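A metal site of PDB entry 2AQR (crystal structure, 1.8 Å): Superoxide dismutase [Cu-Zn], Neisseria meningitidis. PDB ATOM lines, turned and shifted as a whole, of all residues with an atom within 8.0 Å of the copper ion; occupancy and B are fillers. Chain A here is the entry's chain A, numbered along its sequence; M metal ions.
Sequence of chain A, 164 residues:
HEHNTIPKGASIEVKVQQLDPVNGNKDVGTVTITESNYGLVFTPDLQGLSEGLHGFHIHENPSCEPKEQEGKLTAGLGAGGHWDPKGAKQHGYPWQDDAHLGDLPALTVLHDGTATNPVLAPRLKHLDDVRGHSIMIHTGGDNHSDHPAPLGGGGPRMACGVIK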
ATOM      1  N   GLY A  55      36.432   9.361 -11.129  1.00  0.00           N
ATOM      2  CA  GLY A  55      35.141   9.888 -11.559  1.00  0.00           C
ATOM      3  C   GLY A  55      34.803  11.017 -10.613  1.00  0.00           C
ATOM      4  O   GLY A  55      34.964  10.891  -9.394  1.00  0.00           O
ATOM      5  N   PHE A  56      34.283  12.108 -11.162  1.00  0.00           N
ATOM      6  CA  PHE A  56      33.974  13.293 -10.371  1.00  0.00           C
ATOM      7  C   PHE A  56      32.625  13.840 -10.845  1.00  0.00           C
ATOM      8  O   PHE A  56      32.523  14.325 -11.972  1.00  0.00           O
ATOM      9  CB  PHE A  56      35.124  14.283 -10.625  1.00  0.00           C
ATOM     10  CG  PHE A  56      35.170  15.466  -9.703  1.00  0.00           C
ATOM     11  CD1 PHE A  56      34.882  15.338  -8.347  1.00  0.00           C
ATOM     12  CD2 PHE A  56      35.631  16.691 -10.185  1.00  0.00           C
ATOM     13  CE1 PHE A  56      35.053  16.424  -7.482  1.00  0.00           C
ATOM     14  CE2 PHE A  56      35.812  17.773  -9.330  1.00  0.00           C
ATOM     15  CZ  PHE A  56      35.524  17.646  -7.975  1.00  0.00           C
ATOM     16  N   HIS A  57      31.601  13.743 -10.006  1.00  0.00           N
ATOM     17  CA  HIS A  57      30.279  14.220 -10.418  1.00  0.00           C
ATOM     18  C   HIS A  57      29.453  14.838  -9.305  1.00  0.00           C
ATOM     19  O   HIS A  57      29.692  14.612  -8.118  1.00  0.00           O
ATOM     20  CB  HIS A  57      29.429  13.083 -10.990  1.00  0.00           C
ATOM     21  CG  HIS A  57      30.213  11.953 -11.578  1.00  0.00           C
ATOM     22  ND1 HIS A  57      30.378  10.750 -10.936  1.00  0.00           N
ATOM     23  CD2 HIS A  57      30.857  11.835 -12.768  1.00  0.00           C
ATOM     24  CE1 HIS A  57      31.098   9.939 -11.698  1.00  0.00           C
ATOM     25  NE2 HIS A  57      31.386  10.573 -12.815  1.00  0.00           N
ATOM     26  N   ILE A  58      28.466  15.616  -9.720  1.00  0.00           N
ATOM     27  CA  ILE A  58      27.522  16.218  -8.792  1.00  0.00           C
ATOM     28  C   ILE A  58      26.387  15.204  -8.711  1.00  0.00           C
ATOM     29  O   ILE A  58      25.848  14.794  -9.745  1.00  0.00           O
ATOM     30  CB  ILE A  58      26.934  17.538  -9.353  1.00  0.00           C
ATOM     31  CG1 ILE A  58      28.045  18.559  -9.595  1.00  0.00           C
ATOM     32  CG2 ILE A  58      25.887  18.107  -8.383  1.00  0.00           C
ATOM     33  CD1 ILE A  58      28.781  18.983  -8.336  1.00  0.00           C
ATOM     34  N   HIS A  59      26.044  14.771  -7.502  1.00  0.00           N
ATOM     35  CA  HIS A  59      24.946  13.837  -7.329  1.00  0.00           C
ATOM     36  C   HIS A  59      23.712  14.581  -6.835  1.00  0.00           C
ATOM     37  O   HIS A  59      23.824  15.649  -6.241  1.00  0.00           O
ATOM     38  CB  HIS A  59      25.327  12.691  -6.376  1.00  0.00           C
ATOM     39  CG  HIS A  59      26.228  11.680  -7.010  1.00  0.00           C
ATOM     40  ND1 HIS A  59      25.914  10.348  -7.077  1.00  0.00           N
ATOM     41  CD2 HIS A  59      27.416  11.820  -7.637  1.00  0.00           C
ATOM     42  CE1 HIS A  59      26.869   9.702  -7.720  1.00  0.00           C
ATOM     43  NE2 HIS A  59      27.791  10.578  -8.083  1.00  0.00           N
ATOM     44  N   ALA A  79      23.595   9.857  -1.393  1.00  0.00           N
ATOM     45  CA  ALA A  79      23.712  10.958  -2.345  1.00  0.00           C
ATOM     46  C   ALA A  79      22.833  10.777  -3.585  1.00  0.00           C
ATOM     47  O   ALA A  79      22.603  11.733  -4.331  1.00  0.00           O
ATOM     48  CB  ALA A  79      25.169  11.131  -2.774  1.00  0.00           C
ATOM     49  N   GLY A  80      22.345   9.569  -3.807  1.00  0.00           N
ATOM     50  CA  GLY A  80      21.518   9.310  -4.976  1.00  0.00           C
ATOM     51  C   GLY A  80      22.370   9.177  -6.221  1.00  0.00           C
ATOM     52  O   GLY A  80      23.594   8.980  -6.138  1.00  0.00           O
ATOM     53  N   GLY A  81      21.753   9.292  -7.390  1.00  0.00           N
ATOM     54  CA  GLY A  81      22.492   9.154  -8.632  1.00  0.00           C
ATOM     55  C   GLY A  81      23.052  10.467  -9.138  1.00  0.00           C
ATOM     56  O   GLY A  81      23.022  11.486  -8.443  1.00  0.00           O
ATOM     57  N   HIS A  82      23.586  10.453 -10.362  1.00  0.00           N
ATOM     58  CA  HIS A  82      24.140  11.664 -10.932  1.00  0.00           C
ATOM     59  C   HIS A  82      23.041  12.708 -11.107  1.00  0.00           C
ATOM     60  O   HIS A  82      21.932  12.383 -11.558  1.00  0.00           O
ATOM     61  CB  HIS A  82      24.780  11.370 -12.293  1.00  0.00           C
ATOM     62  CG  HIS A  82      25.970  10.466 -12.230  1.00  0.00           C
ATOM     63  ND1 HIS A  82      26.827  10.296 -13.290  1.00  0.00           N
ATOM     64  CD2 HIS A  82      26.440   9.675 -11.235  1.00  0.00           C
ATOM     65  CE1 HIS A  82      27.782   9.448 -12.945  1.00  0.00           C
ATOM     66  NE2 HIS A  82      27.569   9.063 -11.704  1.00  0.00           N
ATOM     67  N   TRP A  83      23.333  13.945 -10.752  1.00  0.00           N
ATOM     68  CA  TRP A  83      22.354  15.015 -10.888  1.00  0.00           C
ATOM     69  C   TRP A  83      21.978  15.146 -12.356  1.00  0.00           C
ATOM     70  O   TRP A  83      22.824  15.418 -13.208  1.00  0.00           O
ATOM     71  CB  TRP A  83      22.922  16.332 -10.342  1.00  0.00           C
ATOM     72  CG  TRP A  83      21.910  17.420 -10.280  1.00  0.00           C
ATOM     73  CD1 TRP A  83      20.619  17.325  -9.846  1.00  0.00           C
ATOM     74  CD2 TRP A  83      22.100  18.791 -10.663  1.00  0.00           C
ATOM     75  NE1 TRP A  83      19.992  18.545  -9.926  1.00  0.00           N
ATOM     76  CE2 TRP A  83      20.884  19.468 -10.417  1.00  0.00           C
ATOM     77  CE3 TRP A  83      23.188  19.508 -11.175  1.00  0.00           C
ATOM     78  CZ2 TRP A  83      20.715  20.832 -10.683  1.00  0.00           C
ATOM     79  CZ3 TRP A  83      23.022  20.871 -11.428  1.00  0.00           C
ATOM     80  CH2 TRP A  83      21.795  21.515 -11.182  1.00  0.00           C
ATOM     81  N   HIS A  91      25.024   9.042 -19.104  1.00  0.00           N
ATOM     82  CA  HIS A  91      26.273   9.589 -18.589  1.00  0.00           C
ATOM     83  C   HIS A  91      27.141  10.004 -19.778  1.00  0.00           C
ATOM     84  O   HIS A  91      27.218   9.273 -20.761  1.00  0.00           O
ATOM     85  CB  HIS A  91      27.010   8.561 -17.751  1.00  0.00           C
ATOM     86  CG  HIS A  91      28.270   9.080 -17.132  1.00  0.00           C
ATOM     87  ND1 HIS A  91      28.261  10.032 -16.134  1.00  0.00           N
ATOM     88  CD2 HIS A  91      29.567   8.845 -17.416  1.00  0.00           C
ATOM     89  CE1 HIS A  91      29.502  10.372 -15.836  1.00  0.00           C
ATOM     90  NE2 HIS A  91      30.313   9.665 -16.603  1.00  0.00           N
ATOM     91  N   GLY A 102      25.322  16.848 -14.030  1.00  0.00           N
ATOM     92  CA  GLY A 102      26.311  16.711 -12.975  1.00  0.00           C
ATOM     93  C   GLY A 102      27.642  16.105 -13.387  1.00  0.00           C
ATOM     94  O   GLY A 102      28.529  15.946 -12.551  1.00  0.00           O
ATOM     95  N   ASP A 103      27.797  15.784 -14.671  1.00  0.00           N
ATOM     96  CA  ASP A 103      29.036  15.166 -15.151  1.00  0.00           C
ATOM     97  C   ASP A 103      30.193  16.166 -15.267  1.00  0.00           C
ATOM     98  O   ASP A 103      30.192  17.038 -16.136  1.00  0.00           O
ATOM     99  CB  ASP A 103      28.813  14.466 -16.500  1.00  0.00           C
ATOM    100  CG  ASP A 103      27.840  13.301 -16.401  1.00  0.00           C
ATOM    101  OD1 ASP A 103      27.611  12.805 -15.273  1.00  0.00           O
ATOM    102  OD2 ASP A 103      27.300  12.880 -17.442  1.00  0.00           O
ATOM    103  N   SER A 134      25.354  17.207  -3.867  1.00  0.00           N
ATOM    104  CA  SER A 134      26.605  16.687  -3.326  1.00  0.00           C
ATOM    105  C   SER A 134      27.621  16.493  -4.445  1.00  0.00           C
ATOM    106  O   SER A 134      27.263  16.430  -5.611  1.00  0.00           O
ATOM    107  CB  SER A 134      26.355  15.350  -2.622  1.00  0.00           C
ATOM    108  OG  SER A 134      25.678  14.440  -3.479  1.00  0.00           O
ATOM    109  N   ILE A 135      28.894  16.440  -4.072  1.00  0.00           N
ATOM    110  CA  ILE A 135      29.936  16.220  -5.054  1.00  0.00           C
ATOM    111  C   ILE A 135      30.593  14.900  -4.661  1.00  0.00           C
ATOM    112  O   ILE A 135      30.898  14.664  -3.496  1.00  0.00           O
ATOM    113  CB  ILE A 135      30.937  17.401  -5.079  1.00  0.00           C
ATOM    114  CG1 ILE A 135      31.920  17.230  -6.240  1.00  0.00           C
ATOM    115  CG2 ILE A 135      31.656  17.520  -3.743  1.00  0.00           C
ATOM    116  CD1 ILE A 135      32.657  18.497  -6.592  1.00  0.00           C
ATOM    117  N   MET A 136      30.761  14.035  -5.651  1.00  0.00           N
ATOM    118  CA  MET A 136      31.298  12.712  -5.399  1.00  0.00           C
ATOM    119  C   MET A 136      32.598  12.406  -6.132  1.00  0.00           C
ATOM    120  O   MET A 136      32.794  12.828  -7.257  1.00  0.00           O
ATOM    121  CB  MET A 136      30.251  11.678  -5.832  1.00  0.00           C
ATOM    122  CG  MET A 136      30.472  10.273  -5.333  1.00  0.00           C
ATOM    123  SD  MET A 136      30.026  10.097  -3.604  1.00  0.00           S
ATOM    124  CE  MET A 136      28.241  10.298  -3.708  1.00  0.00           C
ATOM    125  N   ILE A 137      33.477  11.677  -5.449  1.00  0.00           N
ATOM    126  CA  ILE A 137      34.748  11.242  -6.032  1.00  0.00           C
ATOM    127  C   ILE A 137      34.687   9.717  -5.943  1.00  0.00           C
ATOM    128  O   ILE A 137      34.512   9.147  -4.869  1.00  0.00           O
ATOM    129  CB  ILE A 137      35.950  11.763  -5.226  1.00  0.00           C
ATOM    130  CG1 ILE A 137      35.995  13.294  -5.282  1.00  0.00           C
ATOM    131  CG2 ILE A 137      37.245  11.180  -5.795  1.00  0.00           C
ATOM    132  CD1 ILE A 137      37.116  13.922  -4.479  1.00  0.00           C
ATOM    133  N   HIS A 138      34.822   9.051  -7.087  1.00  0.00           N
ATOM    134  CA  HIS A 138      34.738   7.605  -7.140  1.00  0.00           C
ATOM    135  C   HIS A 138      36.083   6.911  -7.074  1.00  0.00           C
ATOM    136  O   HIS A 138      37.130   7.534  -7.243  1.00  0.00           O
ATOM    137  CB  HIS A 138      34.014   7.171  -8.424  1.00  0.00           C
ATOM    138  CG  HIS A 138      32.575   7.579  -8.467  1.00  0.00           C
ATOM    139  ND1 HIS A 138      31.552   6.719  -8.109  1.00  0.00           N
ATOM    140  CD2 HIS A 138      31.989   8.755  -8.770  1.00  0.00           C
ATOM    141  CE1 HIS A 138      30.397   7.342  -8.207  1.00  0.00           C
ATOM    142  NE2 HIS A 138      30.627   8.584  -8.608  1.00  0.00           N
ATOM    143  N   ASP A 142      36.607   7.600 -15.226  1.00  0.00           N
ATOM    144  CA  ASP A 142      35.432   8.087 -15.939  1.00  0.00           C
ATOM    145  C   ASP A 142      35.736   8.173 -17.439  1.00  0.00           C
ATOM    146  O   ASP A 142      36.503   9.040 -17.862  1.00  0.00           O
ATOM    147  CB  ASP A 142      35.018   9.471 -15.416  1.00  0.00           C
ATOM    148  CG  ASP A 142      33.596   9.848 -15.813  1.00  0.00           C
ATOM    149  OD1 ASP A 142      33.042   9.231 -16.749  1.00  0.00           O
ATOM    150  OD2 ASP A 142      33.034  10.782 -15.202  1.00  0.00           O
ATOM    151  N   LEU A 151      27.814   4.551 -15.893  1.00  0.00           N
ATOM    152  CA  LEU A 151      28.317   5.761 -15.253  1.00  0.00           C
ATOM    153  C   LEU A 151      29.827   5.986 -15.356  1.00  0.00           C
ATOM    154  O   LEU A 151      30.486   6.385 -14.394  1.00  0.00           O
ATOM    155  CB  LEU A 151      27.873   5.760 -13.788  1.00  0.00           C
ATOM    156  CG  LEU A 151      26.364   5.547 -13.626  1.00  0.00           C
ATOM    157  CD1 LEU A 151      26.020   5.281 -12.166  1.00  0.00           C
ATOM    158  CD2 LEU A 151      25.609   6.753 -14.150  1.00  0.00           C
ATOM    159  N   GLY A 154      32.962   4.602 -12.863  1.00  0.00           N
ATOM    160  CA  GLY A 154      33.392   5.152 -11.585  1.00  0.00           C
ATOM    161  C   GLY A 154      33.311   4.138 -10.461  1.00  0.00           C
ATOM    162  O   GLY A 154      34.140   4.133  -9.550  1.00  0.00           O
ATOM    163  N   GLY A 155      32.311   3.267 -10.530  1.00  0.00           N
ATOM    164  CA  GLY A 155      32.164   2.262  -9.485  1.00  0.00           C
ATOM    165  C   GLY A 155      31.867   2.838  -8.123  1.00  0.00           C
ATOM    166  O   GLY A 155      31.141   3.831  -8.008  1.00  0.00           O
ATOM    167  N   PRO A 156      32.425   2.242  -7.054  1.00  0.00           N
ATOM    168  CA  PRO A 156      32.240   2.677  -5.654  1.00  0.00           C
ATOM    169  C   PRO A 156      32.517   4.151  -5.395  1.00  0.00           C
ATOM    170  O   PRO A 156      33.279   4.805  -6.101  1.00  0.00           O
ATOM    171  CB  PRO A 156      33.196   1.770  -4.885  1.00  0.00           C
ATOM    172  CG  PRO A 156      33.226   0.532  -5.711  1.00  0.00           C
ATOM    173  CD  PRO A 156      33.321   1.084  -7.117  1.00  0.00           C
ATOM    174  N   ARG A 157      31.886   4.672  -4.339  1.00  0.00           N
ATOM    175  CA  ARG A 157      32.036   6.061  -3.942  1.00  0.00           C
ATOM    176  C   ARG A 157      33.111   6.157  -2.868  1.00  0.00           C
ATOM    177  O   ARG A 157      32.961   5.646  -1.759  1.00  0.00           O
ATOM    178  CB  ARG A 157      30.680   6.584  -3.465  1.00  0.00           C
ATOM    179  CG  ARG A 157      29.646   6.425  -4.567  1.00  0.00           C
ATOM    180  CD  ARG A 157      28.221   6.746  -4.183  1.00  0.00           C
ATOM    181  NE  ARG A 157      27.334   6.417  -5.286  1.00  0.00           N
ATOM    182  CZ  ARG A 157      26.094   6.868  -5.442  1.00  0.00           C
ATOM    183  NH1 ARG A 157      25.578   7.691  -4.529  1.00  0.00           N
ATOM    184  NH2 ARG A 157      25.377   6.512  -6.498  1.00  0.00           N
ATOM    185  N   ALA A 159      34.968   9.321  -1.916  1.00  0.00           N
ATOM    186  CA  ALA A 159      34.911  10.532  -1.107  1.00  0.00           C
ATOM    187  C   ALA A 159      33.699  11.361  -1.519  1.00  0.00           C
ATOM    188  O   ALA A 159      33.216  11.237  -2.647  1.00  0.00           O
ATOM    189  CB  ALA A 159      36.190  11.332  -1.279  1.00  0.00           C
HETATM  190 CU    CU M   1      29.416  10.126  -9.181  1.00  0.00          CU
HETATM  191 ZN    ZN M   2      26.762  11.075 -15.153  1.00  0.00          ZN
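The copper ion is bound by NE2 of His 59 (2.0 Å). NE2 of His 138 is bound to the copper ion, 2.0 Å away. ND1 of His 57 is bound to the copper ion (2.1 Å).
ND1 of His 138 is in hydrogen-bond range of O of Gly 155 (2.9 Å). A ring nitrogen (NE2) of His 57 is in hydrogen-bond range of the side-chain carboxylate (OD2) of Asp 142, 2.9 Å away. A ring nitrogen (ND1) of His 57 sits close to a ring nitrogen (NE2) of His 82 (3.4 Å). The backbone carbonyl oxygen of His 57 lies within hydrogen-bond range of the backbone NH of Met 136, 2.7 Å away. The backbone carbonyl oxygen (O) of Gly 55 lies within hydrogen-bond range of the backbone NH (N) of His 138, 3.0 Å away. A ring nitrogen (ND1) of His 59 is in hydrogen-bond range of the backbone carbonyl oxygen (O) of Gly 80. A ring nitrogen (ND1) of His 59 lies close to the backbone carbonyl oxygen (O) of Gly 81 (3.4 Å). N of His 59 is in hydrogen-bond range of O of Ser 134.
NE2 of His 82 touches the copper ion, 3.3 Å away. Met 136 touches the copper ion (CB to CU, 3.8 Å). Of the 25 residues printed, 5 come within 4 Å of the copper ion. Along chain A the residues within 4 Å of the copper ion span positions 57 to 138.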
